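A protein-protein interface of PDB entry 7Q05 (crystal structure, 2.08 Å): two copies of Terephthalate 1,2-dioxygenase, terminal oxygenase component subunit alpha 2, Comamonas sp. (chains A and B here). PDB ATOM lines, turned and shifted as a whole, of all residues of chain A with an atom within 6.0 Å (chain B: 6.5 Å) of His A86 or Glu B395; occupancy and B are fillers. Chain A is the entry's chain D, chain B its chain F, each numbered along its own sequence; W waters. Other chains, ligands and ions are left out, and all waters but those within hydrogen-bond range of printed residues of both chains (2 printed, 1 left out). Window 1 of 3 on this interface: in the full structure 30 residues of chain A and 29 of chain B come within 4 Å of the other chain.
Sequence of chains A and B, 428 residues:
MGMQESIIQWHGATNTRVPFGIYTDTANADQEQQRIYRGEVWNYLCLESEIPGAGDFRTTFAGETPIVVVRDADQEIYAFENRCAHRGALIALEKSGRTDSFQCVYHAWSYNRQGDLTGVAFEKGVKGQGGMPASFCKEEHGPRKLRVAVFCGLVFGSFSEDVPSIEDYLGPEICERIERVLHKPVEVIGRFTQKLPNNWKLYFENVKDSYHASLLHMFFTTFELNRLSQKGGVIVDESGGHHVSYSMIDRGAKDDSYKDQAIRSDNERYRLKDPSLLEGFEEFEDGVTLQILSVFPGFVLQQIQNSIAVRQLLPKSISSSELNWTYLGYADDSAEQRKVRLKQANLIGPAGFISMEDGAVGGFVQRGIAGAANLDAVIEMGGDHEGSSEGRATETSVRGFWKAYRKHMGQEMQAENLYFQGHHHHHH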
ATOM      1  N   CYS A  84     -26.549  -2.072   8.444  1.00  0.00           N
ATOM      2  CA  CYS A  84     -26.256  -2.919   9.606  1.00  0.00           C
ATOM      3  C   CYS A  84     -26.813  -2.224  10.847  1.00  0.00           C
ATOM      4  O   CYS A  84     -26.626  -0.977  10.968  1.00  0.00           O
ATOM      5  CB  CYS A  84     -24.764  -3.143   9.713  1.00  0.00           C
ATOM      6  SG  CYS A  84     -24.343  -4.194  11.105  1.00  0.00           S
ATOM      7  N   ALA A  85     -27.419  -2.999  11.751  1.00  0.00           N
ATOM      8  CA  ALA A  85     -28.120  -2.466  12.949  1.00  0.00           C
ATOM      9  C   ALA A  85     -27.108  -2.131  14.033  1.00  0.00           C
ATOM     10  O   ALA A  85     -27.515  -1.619  15.057  1.00  0.00           O
ATOM     11  CB  ALA A  85     -29.139  -3.459  13.430  1.00  0.00           C
ATOM     12  N   HIS A  86     -25.822  -2.413  13.804  1.00  0.00           N
ATOM     13  CA  HIS A  86     -24.740  -2.093  14.772  1.00  0.00           C
ATOM     14  C   HIS A  86     -24.435  -0.600  14.623  1.00  0.00           C
ATOM     15  O   HIS A  86     -25.063   0.187  15.322  1.00  0.00           O
ATOM     16  CB  HIS A  86     -23.538  -3.039  14.562  1.00  0.00           C
ATOM     17  CG  HIS A  86     -22.377  -2.720  15.436  1.00  0.00           C
ATOM     18  ND1 HIS A  86     -21.062  -2.787  14.990  1.00  0.00           N
ATOM     19  CD2 HIS A  86     -22.330  -2.283  16.714  1.00  0.00           C
ATOM     20  CE1 HIS A  86     -20.261  -2.452  15.978  1.00  0.00           C
ATOM     21  NE2 HIS A  86     -21.017  -2.129  17.063  1.00  0.00           N
ATOM     22  N   ARG A  87     -23.592  -0.228  13.653  1.00  0.00           N
ATOM     23  CA  ARG A  87     -23.109   1.175  13.485  1.00  0.00           C
ATOM     24  C   ARG A  87     -23.454   1.695  12.082  1.00  0.00           C
ATOM     25  O   ARG A  87     -22.972   2.770  11.757  1.00  0.00           O
ATOM     26  CB  ARG A  87     -21.627   1.278  13.889  1.00  0.00           C
ATOM     27  CG  ARG A  87     -21.412   1.083  15.381  1.00  0.00           C
ATOM     28  CD  ARG A  87     -20.061   1.398  16.003  1.00  0.00           C
ATOM     29  NE  ARG A  87     -19.570   2.590  15.354  1.00  0.00           N
ATOM     30  CZ  ARG A  87     -18.398   2.690  14.706  1.00  0.00           C
ATOM     31  NH1 ARG A  87     -17.504   1.701  14.749  1.00  0.00           N
ATOM     32  NH2 ARG A  87     -18.132   3.819  14.042  1.00  0.00           N
ATOM     33  N   GLY A  88     -24.310   1.012  11.321  1.00  0.00           N
ATOM     34  CA  GLY A  88     -24.909   1.546  10.086  1.00  0.00           C
ATOM     35  C   GLY A  88     -24.194   1.195   8.757  1.00  0.00           C
ATOM     36  O   GLY A  88     -24.602   1.723   7.712  1.00  0.00           O
ATOM     37  N   TYR A 106     -17.698  -5.063   8.831  1.00  0.00           N
ATOM     38  CA  TYR A 106     -17.085  -4.164   9.846  1.00  0.00           C
ATOM     39  C   TYR A 106     -16.860  -4.959  11.141  1.00  0.00           C
ATOM     40  O   TYR A 106     -15.717  -5.025  11.583  1.00  0.00           O
ATOM     41  CB  TYR A 106     -17.949  -2.918  10.038  1.00  0.00           C
ATOM     42  CG  TYR A 106     -17.244  -1.715  10.604  1.00  0.00           C
ATOM     43  CD1 TYR A 106     -15.961  -1.790  11.095  1.00  0.00           C
ATOM     44  CD2 TYR A 106     -17.885  -0.489  10.644  1.00  0.00           C
ATOM     45  CE1 TYR A 106     -15.325  -0.685  11.612  1.00  0.00           C
ATOM     46  CE2 TYR A 106     -17.260   0.624  11.161  1.00  0.00           C
ATOM     47  CZ  TYR A 106     -15.962   0.540  11.637  1.00  0.00           C
ATOM     48  OH  TYR A 106     -15.298   1.657  12.138  1.00  0.00           O
ATOM     49  N   HIS A 107     -17.910  -5.542  11.740  1.00  0.00           N
ATOM     50  CA  HIS A 107     -17.749  -6.345  12.991  1.00  0.00           C
ATOM     51  C   HIS A 107     -18.450  -7.698  12.902  1.00  0.00           C
ATOM     52  O   HIS A 107     -18.750  -8.266  13.976  1.00  0.00           O
ATOM     53  CB  HIS A 107     -18.222  -5.579  14.225  1.00  0.00           C
ATOM     54  CG  HIS A 107     -17.799  -4.158  14.255  1.00  0.00           C
ATOM     55  ND1 HIS A 107     -18.457  -3.195  13.533  1.00  0.00           N
ATOM     56  CD2 HIS A 107     -16.809  -3.535  14.932  1.00  0.00           C
ATOM     57  CE1 HIS A 107     -17.889  -2.024  13.754  1.00  0.00           C
ATOM     58  NE2 HIS A 107     -16.851  -2.205  14.601  1.00  0.00           N
ATOM     59  N   TRP A 109     -21.370  -8.914  12.082  1.00  0.00           N
ATOM     60  CA  TRP A 109     -22.782  -9.223  12.435  1.00  0.00           C
ATOM     61  C   TRP A 109     -23.400  -9.953  11.227  1.00  0.00           C
ATOM     62  O   TRP A 109     -23.185  -9.508  10.087  1.00  0.00           O
ATOM     63  CB  TRP A 109     -23.582  -7.968  12.836  1.00  0.00           C
ATOM     64  CG  TRP A 109     -23.202  -7.400  14.169  1.00  0.00           C
ATOM     65  CD1 TRP A 109     -21.997  -7.511  14.787  1.00  0.00           C
ATOM     66  CD2 TRP A 109     -24.017  -6.607  15.046  1.00  0.00           C
ATOM     67  NE1 TRP A 109     -22.003  -6.836  15.974  1.00  0.00           N
ATOM     68  CE2 TRP A 109     -23.222  -6.268  16.159  1.00  0.00           C
ATOM     69  CE3 TRP A 109     -25.328  -6.127  14.991  1.00  0.00           C
ATOM     70  CZ2 TRP A 109     -23.700  -5.503  17.223  1.00  0.00           C
ATOM     71  CZ3 TRP A 109     -25.805  -5.369  16.037  1.00  0.00           C
ATOM     72  CH2 TRP A 109     -25.004  -5.072  17.147  1.00  0.00           C
ATOM     73  N   TYR A 111     -26.856 -11.679   9.226  1.00  0.00           N
ATOM     74  CA  TYR A 111     -28.295 -11.499   8.940  1.00  0.00           C
ATOM     75  C   TYR A 111     -28.757 -12.688   8.088  1.00  0.00           C
ATOM     76  O   TYR A 111     -27.992 -13.105   7.185  1.00  0.00           O
ATOM     77  CB  TYR A 111     -28.514 -10.141   8.258  1.00  0.00           C
ATOM     78  CG  TYR A 111     -28.048  -8.987   9.111  1.00  0.00           C
ATOM     79  CD1 TYR A 111     -26.716  -8.559   9.074  1.00  0.00           C
ATOM     80  CD2 TYR A 111     -28.924  -8.323   9.967  1.00  0.00           C
ATOM     81  CE1 TYR A 111     -26.269  -7.537   9.895  1.00  0.00           C
ATOM     82  CE2 TYR A 111     -28.489  -7.276  10.769  1.00  0.00           C
ATOM     83  CZ  TYR A 111     -27.156  -6.883  10.744  1.00  0.00           C
ATOM     84  OH  TYR A 111     -26.726  -5.848  11.528  1.00  0.00           O
ATOM     85  N   MET A 132     -21.657  -7.951  24.846  1.00  0.00           N
ATOM     86  CA  MET A 132     -22.921  -7.197  25.146  1.00  0.00           C
ATOM     87  C   MET A 132     -23.354  -7.344  26.611  1.00  0.00           C
ATOM     88  O   MET A 132     -23.023  -8.316  27.281  1.00  0.00           O
ATOM     89  CB  MET A 132     -24.013  -7.686  24.196  1.00  0.00           C
ATOM     90  CG  MET A 132     -23.661  -7.410  22.764  1.00  0.00           C
ATOM     91  SD  MET A 132     -23.280  -5.639  22.540  1.00  0.00           S
ATOM     92  CE  MET A 132     -23.540  -5.384  20.784  1.00  0.00           C
ATOM     93  N   PHE B  20     -27.239   9.292  14.133  1.00  0.00           N
ATOM     94  CA  PHE B  20     -26.613   9.205  12.796  1.00  0.00           C
ATOM     95  C   PHE B  20     -26.567  10.590  12.144  1.00  0.00           C
ATOM     96  O   PHE B  20     -25.684  10.854  11.330  1.00  0.00           O
ATOM     97  CB  PHE B  20     -27.377   8.201  11.928  1.00  0.00           C
ATOM     98  CG  PHE B  20     -27.060   6.756  12.208  1.00  0.00           C
ATOM     99  CD1 PHE B  20     -25.753   6.337  12.436  1.00  0.00           C
ATOM    100  CD2 PHE B  20     -28.077   5.806  12.185  1.00  0.00           C
ATOM    101  CE1 PHE B  20     -25.466   4.996  12.624  1.00  0.00           C
ATOM    102  CE2 PHE B  20     -27.790   4.467  12.380  1.00  0.00           C
ATOM    103  CZ  PHE B  20     -26.479   4.072  12.599  1.00  0.00           C
ATOM    104  N   LYS B 208     -10.313   3.960  17.253  1.00  0.00           N
ATOM    105  CA  LYS B 208     -10.602   3.632  18.669  1.00  0.00           C
ATOM    106  C   LYS B 208     -11.358   2.298  18.759  1.00  0.00           C
ATOM    107  O   LYS B 208     -11.651   1.841  19.902  1.00  0.00           O
ATOM    108  CB  LYS B 208     -11.384   4.796  19.293  1.00  0.00           C
ATOM    109  CG  LYS B 208     -10.601   6.115  19.358  1.00  0.00           C
ATOM    110  CD  LYS B 208     -11.487   7.281  19.732  1.00  0.00           C
ATOM    111  CE  LYS B 208     -10.726   8.556  19.953  1.00  0.00           C
ATOM    112  NZ  LYS B 208      -9.818   8.422  21.119  1.00  0.00           N
ATOM    113  N   ASP B 209     -11.655   1.666  17.626  1.00  0.00           N
ATOM    114  CA  ASP B 209     -12.602   0.528  17.575  1.00  0.00           C
ATOM    115  C   ASP B 209     -11.820  -0.779  17.769  1.00  0.00           C
ATOM    116  O   ASP B 209     -11.557  -1.497  16.779  1.00  0.00           O
ATOM    117  CB  ASP B 209     -13.440   0.606  16.302  1.00  0.00           C
ATOM    118  CG  ASP B 209     -14.591  -0.374  16.219  1.00  0.00           C
ATOM    119  OD1 ASP B 209     -14.661  -1.310  17.057  1.00  0.00           O
ATOM    120  OD2 ASP B 209     -15.371  -0.218  15.273  1.00  0.00           O
ATOM    121  N   SER B 210     -11.550  -1.122  19.022  1.00  0.00           N
ATOM    122  CA  SER B 210     -10.798  -2.340  19.399  1.00  0.00           C
ATOM    123  C   SER B 210     -11.584  -3.586  18.981  1.00  0.00           C
ATOM    124  O   SER B 210     -10.963  -4.583  18.661  1.00  0.00           O
ATOM    125  CB  SER B 210     -10.494  -2.308  20.892  1.00  0.00           C
ATOM    126  OG  SER B 210     -11.687  -2.356  21.659  1.00  0.00           O
ATOM    127  N   TYR B 211     -12.916  -3.499  18.961  1.00  0.00           N
ATOM    128  CA  TYR B 211     -13.846  -4.575  18.539  1.00  0.00           C
ATOM    129  C   TYR B 211     -13.552  -5.007  17.090  1.00  0.00           C
ATOM    130  O   TYR B 211     -13.364  -6.201  16.801  1.00  0.00           O
ATOM    131  CB  TYR B 211     -15.274  -4.048  18.689  1.00  0.00           C
ATOM    132  CG  TYR B 211     -16.412  -4.964  18.346  1.00  0.00           C
ATOM    133  CD1 TYR B 211     -16.253  -6.335  18.368  1.00  0.00           C
ATOM    134  CD2 TYR B 211     -17.666  -4.446  18.055  1.00  0.00           C
ATOM    135  CE1 TYR B 211     -17.313  -7.177  18.105  1.00  0.00           C
ATOM    136  CE2 TYR B 211     -18.743  -5.282  17.805  1.00  0.00           C
ATOM    137  CZ  TYR B 211     -18.564  -6.657  17.838  1.00  0.00           C
ATOM    138  OH  TYR B 211     -19.584  -7.532  17.611  1.00  0.00           O
ATOM    139  N   ASP B 376     -30.121   5.709  15.220  1.00  0.00           N
ATOM    140  CA  ASP B 376     -29.032   5.727  16.227  1.00  0.00           C
ATOM    141  C   ASP B 376     -28.100   4.527  16.005  1.00  0.00           C
ATOM    142  O   ASP B 376     -28.581   3.386  15.816  1.00  0.00           O
ATOM    143  CB  ASP B 376     -29.609   5.671  17.652  1.00  0.00           C
ATOM    144  CG  ASP B 376     -30.271   6.945  18.171  1.00  0.00           C
ATOM    145  OD1 ASP B 376     -29.924   8.000  17.711  1.00  0.00           O
ATOM    146  OD2 ASP B 376     -31.128   6.844  19.066  1.00  0.00           O
ATOM    147  N   ALA B 377     -26.801   4.776  16.064  1.00  0.00           N
ATOM    148  CA  ALA B 377     -25.785   3.718  16.195  1.00  0.00           C
ATOM    149  C   ALA B 377     -25.957   3.059  17.562  1.00  0.00           C
ATOM    150  O   ALA B 377     -26.295   3.748  18.518  1.00  0.00           O
ATOM    151  CB  ALA B 377     -24.404   4.310  16.040  1.00  0.00           C
ATOM    152  N   VAL B 378     -25.695   1.763  17.648  1.00  0.00           N
ATOM    153  CA  VAL B 378     -25.728   0.979  18.914  1.00  0.00           C
ATOM    154  C   VAL B 378     -24.282   0.672  19.320  1.00  0.00           C
ATOM    155  O   VAL B 378     -23.576  -0.051  18.562  1.00  0.00           O
ATOM    156  CB  VAL B 378     -26.549  -0.299  18.723  1.00  0.00           C
ATOM    157  CG1 VAL B 378     -26.331  -1.262  19.868  1.00  0.00           C
ATOM    158  CG2 VAL B 378     -28.028   0.015  18.498  1.00  0.00           C
ATOM    159  N   ILE B 379     -23.858   1.192  20.471  1.00  0.00           N
ATOM    160  CA  ILE B 379     -22.458   1.061  20.984  1.00  0.00           C
ATOM    161  C   ILE B 379     -22.489   0.536  22.422  1.00  0.00           C
ATOM    162  O   ILE B 379     -22.240   1.326  23.344  1.00  0.00           O
ATOM    163  CB  ILE B 379     -21.753   2.418  20.884  1.00  0.00           C
ATOM    164  CG1 ILE B 379     -22.035   3.088  19.531  1.00  0.00           C
ATOM    165  CG2 ILE B 379     -20.275   2.241  21.160  1.00  0.00           C
ATOM    166  CD1 ILE B 379     -21.271   4.343  19.286  1.00  0.00           C
ATOM    167  N   GLU B 380     -22.771  -0.747  22.599  1.00  0.00           N
ATOM    168  CA  GLU B 380     -23.078  -1.334  23.918  1.00  0.00           C
ATOM    169  C   GLU B 380     -22.038  -2.366  24.339  1.00  0.00           C
ATOM    170  O   GLU B 380     -22.150  -2.938  25.434  1.00  0.00           O
ATOM    171  CB  GLU B 380     -24.430  -2.036  23.875  1.00  0.00           C
ATOM    172  CG  GLU B 380     -25.560  -1.110  24.201  1.00  0.00           C
ATOM    173  CD  GLU B 380     -26.897  -1.790  24.200  1.00  0.00           C
ATOM    174  OE1 GLU B 380     -26.976  -2.991  24.554  1.00  0.00           O
ATOM    175  OE2 GLU B 380     -27.839  -1.123  23.787  1.00  0.00           O
ATOM    176  N   MET B 381     -21.087  -2.657  23.487  1.00  0.00           N
ATOM    177  CA  MET B 381     -20.074  -3.705  23.732  1.00  0.00           C
ATOM    178  C   MET B 381     -19.165  -3.252  24.895  1.00  0.00           C
ATOM    179  O   MET B 381     -18.612  -2.137  24.838  1.00  0.00           O
ATOM    180  CB  MET B 381     -19.325  -3.860  22.406  1.00  0.00           C
ATOM    181  CG  MET B 381     -18.849  -5.200  22.090  1.00  0.00           C
ATOM    182  SD  MET B 381     -20.114  -6.422  21.775  1.00  0.00           S
ATOM    183  CE  MET B 381     -18.874  -7.637  21.355  1.00  0.00           C
ATOM    184  N   GLY B 382     -19.044  -4.067  25.949  1.00  0.00           N
ATOM    185  CA  GLY B 382     -18.310  -3.715  27.184  1.00  0.00           C
ATOM    186  C   GLY B 382     -19.098  -2.785  28.109  1.00  0.00           C
ATOM    187  O   GLY B 382     -18.445  -2.115  28.916  1.00  0.00           O
ATOM    188  N   GLY B 383     -20.430  -2.718  27.963  1.00  0.00           N
ATOM    189  CA  GLY B 383     -21.360  -1.945  28.819  1.00  0.00           C
ATOM    190  C   GLY B 383     -21.617  -0.513  28.336  1.00  0.00           C
ATOM    191  O   GLY B 383     -21.682  -0.285  27.107  1.00  0.00           O
ATOM    192  N   HIS B 385     -19.642   1.905  29.879  1.00  0.00           N
ATOM    193  CA  HIS B 385     -18.314   2.347  30.377  1.00  0.00           C
ATOM    194  C   HIS B 385     -17.624   3.246  29.357  1.00  0.00           C
ATOM    195  O   HIS B 385     -17.764   2.911  28.173  1.00  0.00           O
ATOM    196  CB  HIS B 385     -17.439   1.089  30.584  1.00  0.00           C
ATOM    197  CG  HIS B 385     -16.639   1.113  31.843  1.00  0.00           C
ATOM    198  ND1 HIS B 385     -15.266   1.212  31.834  1.00  0.00           N
ATOM    199  CD2 HIS B 385     -17.012   1.015  33.153  1.00  0.00           C
ATOM    200  CE1 HIS B 385     -14.814   1.192  33.084  1.00  0.00           C
ATOM    201  NE2 HIS B 385     -15.873   1.070  33.917  1.00  0.00           N
ATOM    202  N   ARG B 392     -10.246  -6.538  24.429  1.00  0.00           N
ATOM    203  CA  ARG B 392     -10.517  -5.575  23.342  1.00  0.00           C
ATOM    204  C   ARG B 392     -11.886  -5.800  22.692  1.00  0.00           C
ATOM    205  O   ARG B 392     -12.230  -4.994  21.850  1.00  0.00           O
ATOM    206  CB  ARG B 392      -9.339  -5.707  22.371  1.00  0.00           C
ATOM    207  CG  ARG B 392      -8.081  -5.037  22.900  1.00  0.00           C
ATOM    208  CD  ARG B 392      -6.827  -5.857  22.696  1.00  0.00           C
ATOM    209  NE  ARG B 392      -6.520  -6.118  21.294  1.00  0.00           N
ATOM    210  CZ  ARG B 392      -6.122  -7.295  20.802  1.00  0.00           C
ATOM    211  NH1 ARG B 392      -5.836  -7.410  19.516  1.00  0.00           N
ATOM    212  NH2 ARG B 392      -6.064  -8.363  21.581  1.00  0.00           N
ATOM    213  N   ALA B 393     -12.664  -6.793  23.127  1.00  0.00           N
ATOM    214  CA  ALA B 393     -14.081  -7.036  22.733  1.00  0.00           C
ATOM    215  C   ALA B 393     -14.995  -6.071  23.514  1.00  0.00           C
ATOM    216  O   ALA B 393     -15.946  -6.499  24.193  1.00  0.00           O
ATOM    217  CB  ALA B 393     -14.420  -8.486  22.947  1.00  0.00           C
ATOM    218  N   THR B 394     -14.737  -4.774  23.340  1.00  0.00           N
ATOM    219  CA  THR B 394     -15.432  -3.647  24.000  1.00  0.00           C
ATOM    220  C   THR B 394     -15.472  -2.475  23.028  1.00  0.00           C
ATOM    221  O   THR B 394     -14.630  -2.453  22.128  1.00  0.00           O
ATOM    222  CB  THR B 394     -14.684  -3.263  25.280  1.00  0.00           C
ATOM    223  OG1 THR B 394     -15.355  -2.143  25.859  1.00  0.00           O
ATOM    224  CG2 THR B 394     -13.228  -2.914  25.031  1.00  0.00           C
ATOM    225  N   GLU B 395     -16.385  -1.522  23.244  1.00  0.00           N
ATOM    226  CA  GLU B 395     -16.414  -0.229  22.510  1.00  0.00           C
ATOM    227  C   GLU B 395     -16.183   0.936  23.479  1.00  0.00           C
ATOM    228  O   GLU B 395     -16.603   2.081  23.159  1.00  0.00           O
ATOM    229  CB  GLU B 395     -17.738  -0.102  21.760  1.00  0.00           C
ATOM    230  CG  GLU B 395     -17.815  -1.013  20.543  1.00  0.00           C
ATOM    231  CD  GLU B 395     -19.229  -1.235  20.029  1.00  0.00           C
ATOM    232  OE1 GLU B 395     -20.124  -1.550  20.853  1.00  0.00           O
ATOM    233  OE2 GLU B 395     -19.452  -1.031  18.798  1.00  0.00           O
ATOM    234  N   THR B 396     -15.528   0.677  24.612  1.00  0.00           N
ATOM    235  CA  THR B 396     -15.313   1.677  25.688  1.00  0.00           C
ATOM    236  C   THR B 396     -14.586   2.909  25.139  1.00  0.00           C
ATOM    237  O   THR B 396     -15.016   4.026  25.488  1.00  0.00           O
ATOM    238  CB  THR B 396     -14.609   1.067  26.905  1.00  0.00           C
ATOM    239  OG1 THR B 396     -14.595   2.088  27.894  1.00  0.00           O
ATOM    240  CG2 THR B 396     -13.205   0.588  26.612  1.00  0.00           C
ATOM    241  N   SER B 397     -13.556   2.740  24.297  1.00  0.00           N
ATOM    242  CA  SER B 397     -12.782   3.876  23.722  1.00  0.00           C
ATOM    243  C   SER B 397     -13.619   4.630  22.678  1.00  0.00           C
ATOM    244  O   SER B 397     -13.393   5.840  22.481  1.00  0.00           O
ATOM    245  CB  SER B 397     -11.438   3.416  23.148  1.00  0.00           C
ATOM    246  OG  SER B 397     -11.532   2.172  22.480  1.00  0.00           O
ATOM    247  N   VAL B 398     -14.577   3.969  22.026  1.00  0.00           N
ATOM    248  CA  VAL B 398     -15.510   4.663  21.106  1.00  0.00           C
ATOM    249  C   VAL B 398     -16.479   5.529  21.935  1.00  0.00           C
ATOM    250  O   VAL B 398     -16.669   6.703  21.584  1.00  0.00           O
ATOM    251  CB  VAL B 398     -16.239   3.688  20.175  1.00  0.00           C
ATOM    252  CG1 VAL B 398     -17.189   4.456  19.248  1.00  0.00           C
ATOM    253  CG2 VAL B 398     -15.241   2.833  19.386  1.00  0.00           C
ATOM    254  N   ARG B 399     -17.082   4.970  22.974  1.00  0.00           N
ATOM    255  CA  ARG B 399     -17.972   5.752  23.881  1.00  0.00           C
ATOM    256  C   ARG B 399     -17.155   6.942  24.444  1.00  0.00           C
ATOM    257  O   ARG B 399     -17.678   8.078  24.487  1.00  0.00           O
ATOM    258  CB  ARG B 399     -18.590   4.832  24.939  1.00  0.00           C
ATOM    259  CG  ARG B 399     -19.652   3.887  24.400  1.00  0.00           C
ATOM    260  CD  ARG B 399     -20.426   3.179  25.497  1.00  0.00           C
ATOM    261  NE  ARG B 399     -19.545   2.274  26.223  1.00  0.00           N
ATOM    262  CZ  ARG B 399     -19.250   1.021  25.871  1.00  0.00           C
ATOM    263  NH1 ARG B 399     -19.808   0.478  24.804  1.00  0.00           N
ATOM    264  NH2 ARG B 399     -18.430   0.296  26.610  1.00  0.00           N
ATOM    265  N   GLY B 400     -15.894   6.713  24.798  1.00  0.00           N
ATOM    266  CA  GLY B 400     -15.020   7.768  25.336  1.00  0.00           C
ATOM    267  C   GLY B 400     -14.967   8.958  24.387  1.00  0.00           C
ATOM    268  O   GLY B 400     -15.004  10.130  24.847  1.00  0.00           O
HETATM  269  O   HOH W   1     -22.466  -2.193  20.136  1.00  0.00           O
HETATM  270  O   HOH W   2     -17.521  -0.049  17.119  1.00  0.00           O
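Val B378 touches Ala A85 (CG2 to O, 3.8 Å).
His A86 touches Tyr B211 (CE1 to CE2, 3.7 Å).
Ala B377 touches His A86.
O of Arg A87 touches CE1 of Phe B20 (3.5 Å).
OE2 of Glu B395 touches CD of Arg A87 (3.8 Å).
CA of Gly A88 touches CZ of Phe B20, at 3.9 Å.
Tyr A106 touches Asp B209 (OH to OD2, 3.7 Å).
CD2 of Tyr B211 touches CD2 of His A107, 3.4 Å away.
Met A132 touches Glu B380.
Of chain B, only Tyr B211 (3.7 Å), Ala B377 (3.7 Å), Val B378 (2.9 Å) and Glu B395 (2.6 Å) come within 4 Å of His A86.
Of the printed residues of chain B, Gly A88 touches Phe B20.
Of the printed residues of chain B, Tyr A106 touches Asp B209 (3.7 Å).
Printed residues of chain B within 4 Å of Met A132: Glu B380 and Met B381.
The nearest residue of chain B that does not touch His A86 is Asp B376 (4.8 Å).
Water W1 lies within hydrogen-bond range of the side-chain carboxylate of Glu B395 (2.5 Å), the backbone NH of Glu B380 (2.9 Å), the backbone carbonyl oxygen of Val B378 (2.9 Å) and a ring nitrogen (NE2) of His A86 (3.4 Å).
Water W2 lies within hydrogen-bond range of OE2 of Glu B395 (2.7 Å), OD2 of Asp B209 (2.8 Å), NH1 of Arg A87 (2.9 Å) and NE2 of His A107 (3.4 Å).
The side-chain hydroxyl of Tyr A106 sits at hydrogen-bond distance from the guanidinium group of Arg A87, 3.4 Å away.
SG of Cys A84 lies close to N of His A86, at 3.6 Å.
O of Met B381 sits at hydrogen-bond distance from N of Glu B395, at 2.8 Å.
The backbone NH (N) of Tyr B211 sits close to the side-chain carboxylate (OD1) of Asp B209 (3.4 Å).
The backbone carbonyl oxygen (O) of Arg B392 sits at hydrogen-bond distance from the backbone NH (N) of Tyr B211 (3.3 Å).
OH of Tyr A111 lies within hydrogen-bond range of N of Ala A85, 2.9 Å away.
No position is printed for both chains.
Of the 15 pairs that touch across the chains among the printed residues, none has its exchanged pair printed and touching as well.
Of the 23 printed residues of chain B, 8 touch a printed residue of chain A.
Printed residues of chain B that touch a printed residue of chain A: Phe B20, Asp B209, Tyr B211, Ala B377, Val B378, Glu B380, Met B381 and Glu B395.
Hydrophobic or aromatic side chains of chain B that line the printed part of chain A: Phe B20, Tyr B211, Val B378 and Met B381.
Of the 10 printed residues of chain A, 8 touch a printed residue of chain B.
Hydrophobic or aromatic side chains of chain A that line the printed part of chain B: His A86, Tyr A106, His A107, Trp A109 and Met A132.
Among the printed residues, Asp or Glu carboxylates within 4 Å of a Lys or Arg side-chain nitrogen of the other chain: Arg A87 with Asp B209 (2.9 Å).
O of His A86 lies within hydrogen-bond range of N of Val B378 (2.9 Å).
NE2 of His A107 lies within hydrogen-bond range of OD2 of Asp B209 (2.6 Å).
The side-chain sulfur (SD) of Met B381 lies close to the backbone NH (N) of Met A132 (3.8 Å).
The indole nitrogen (NE1) of Trp A109 sits at hydrogen-bond distance from the side-chain hydroxyl (OH) of Tyr B211 (3.0 Å).
A ring nitrogen (NE2) of His A86 sits at hydrogen-bond distance from the side-chain carboxylate (OE2) of Glu B395 (2.6 Å).
NH1 of Arg A87 lies within salt-bridge range of OD2 of Asp B209 (2.9 Å).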
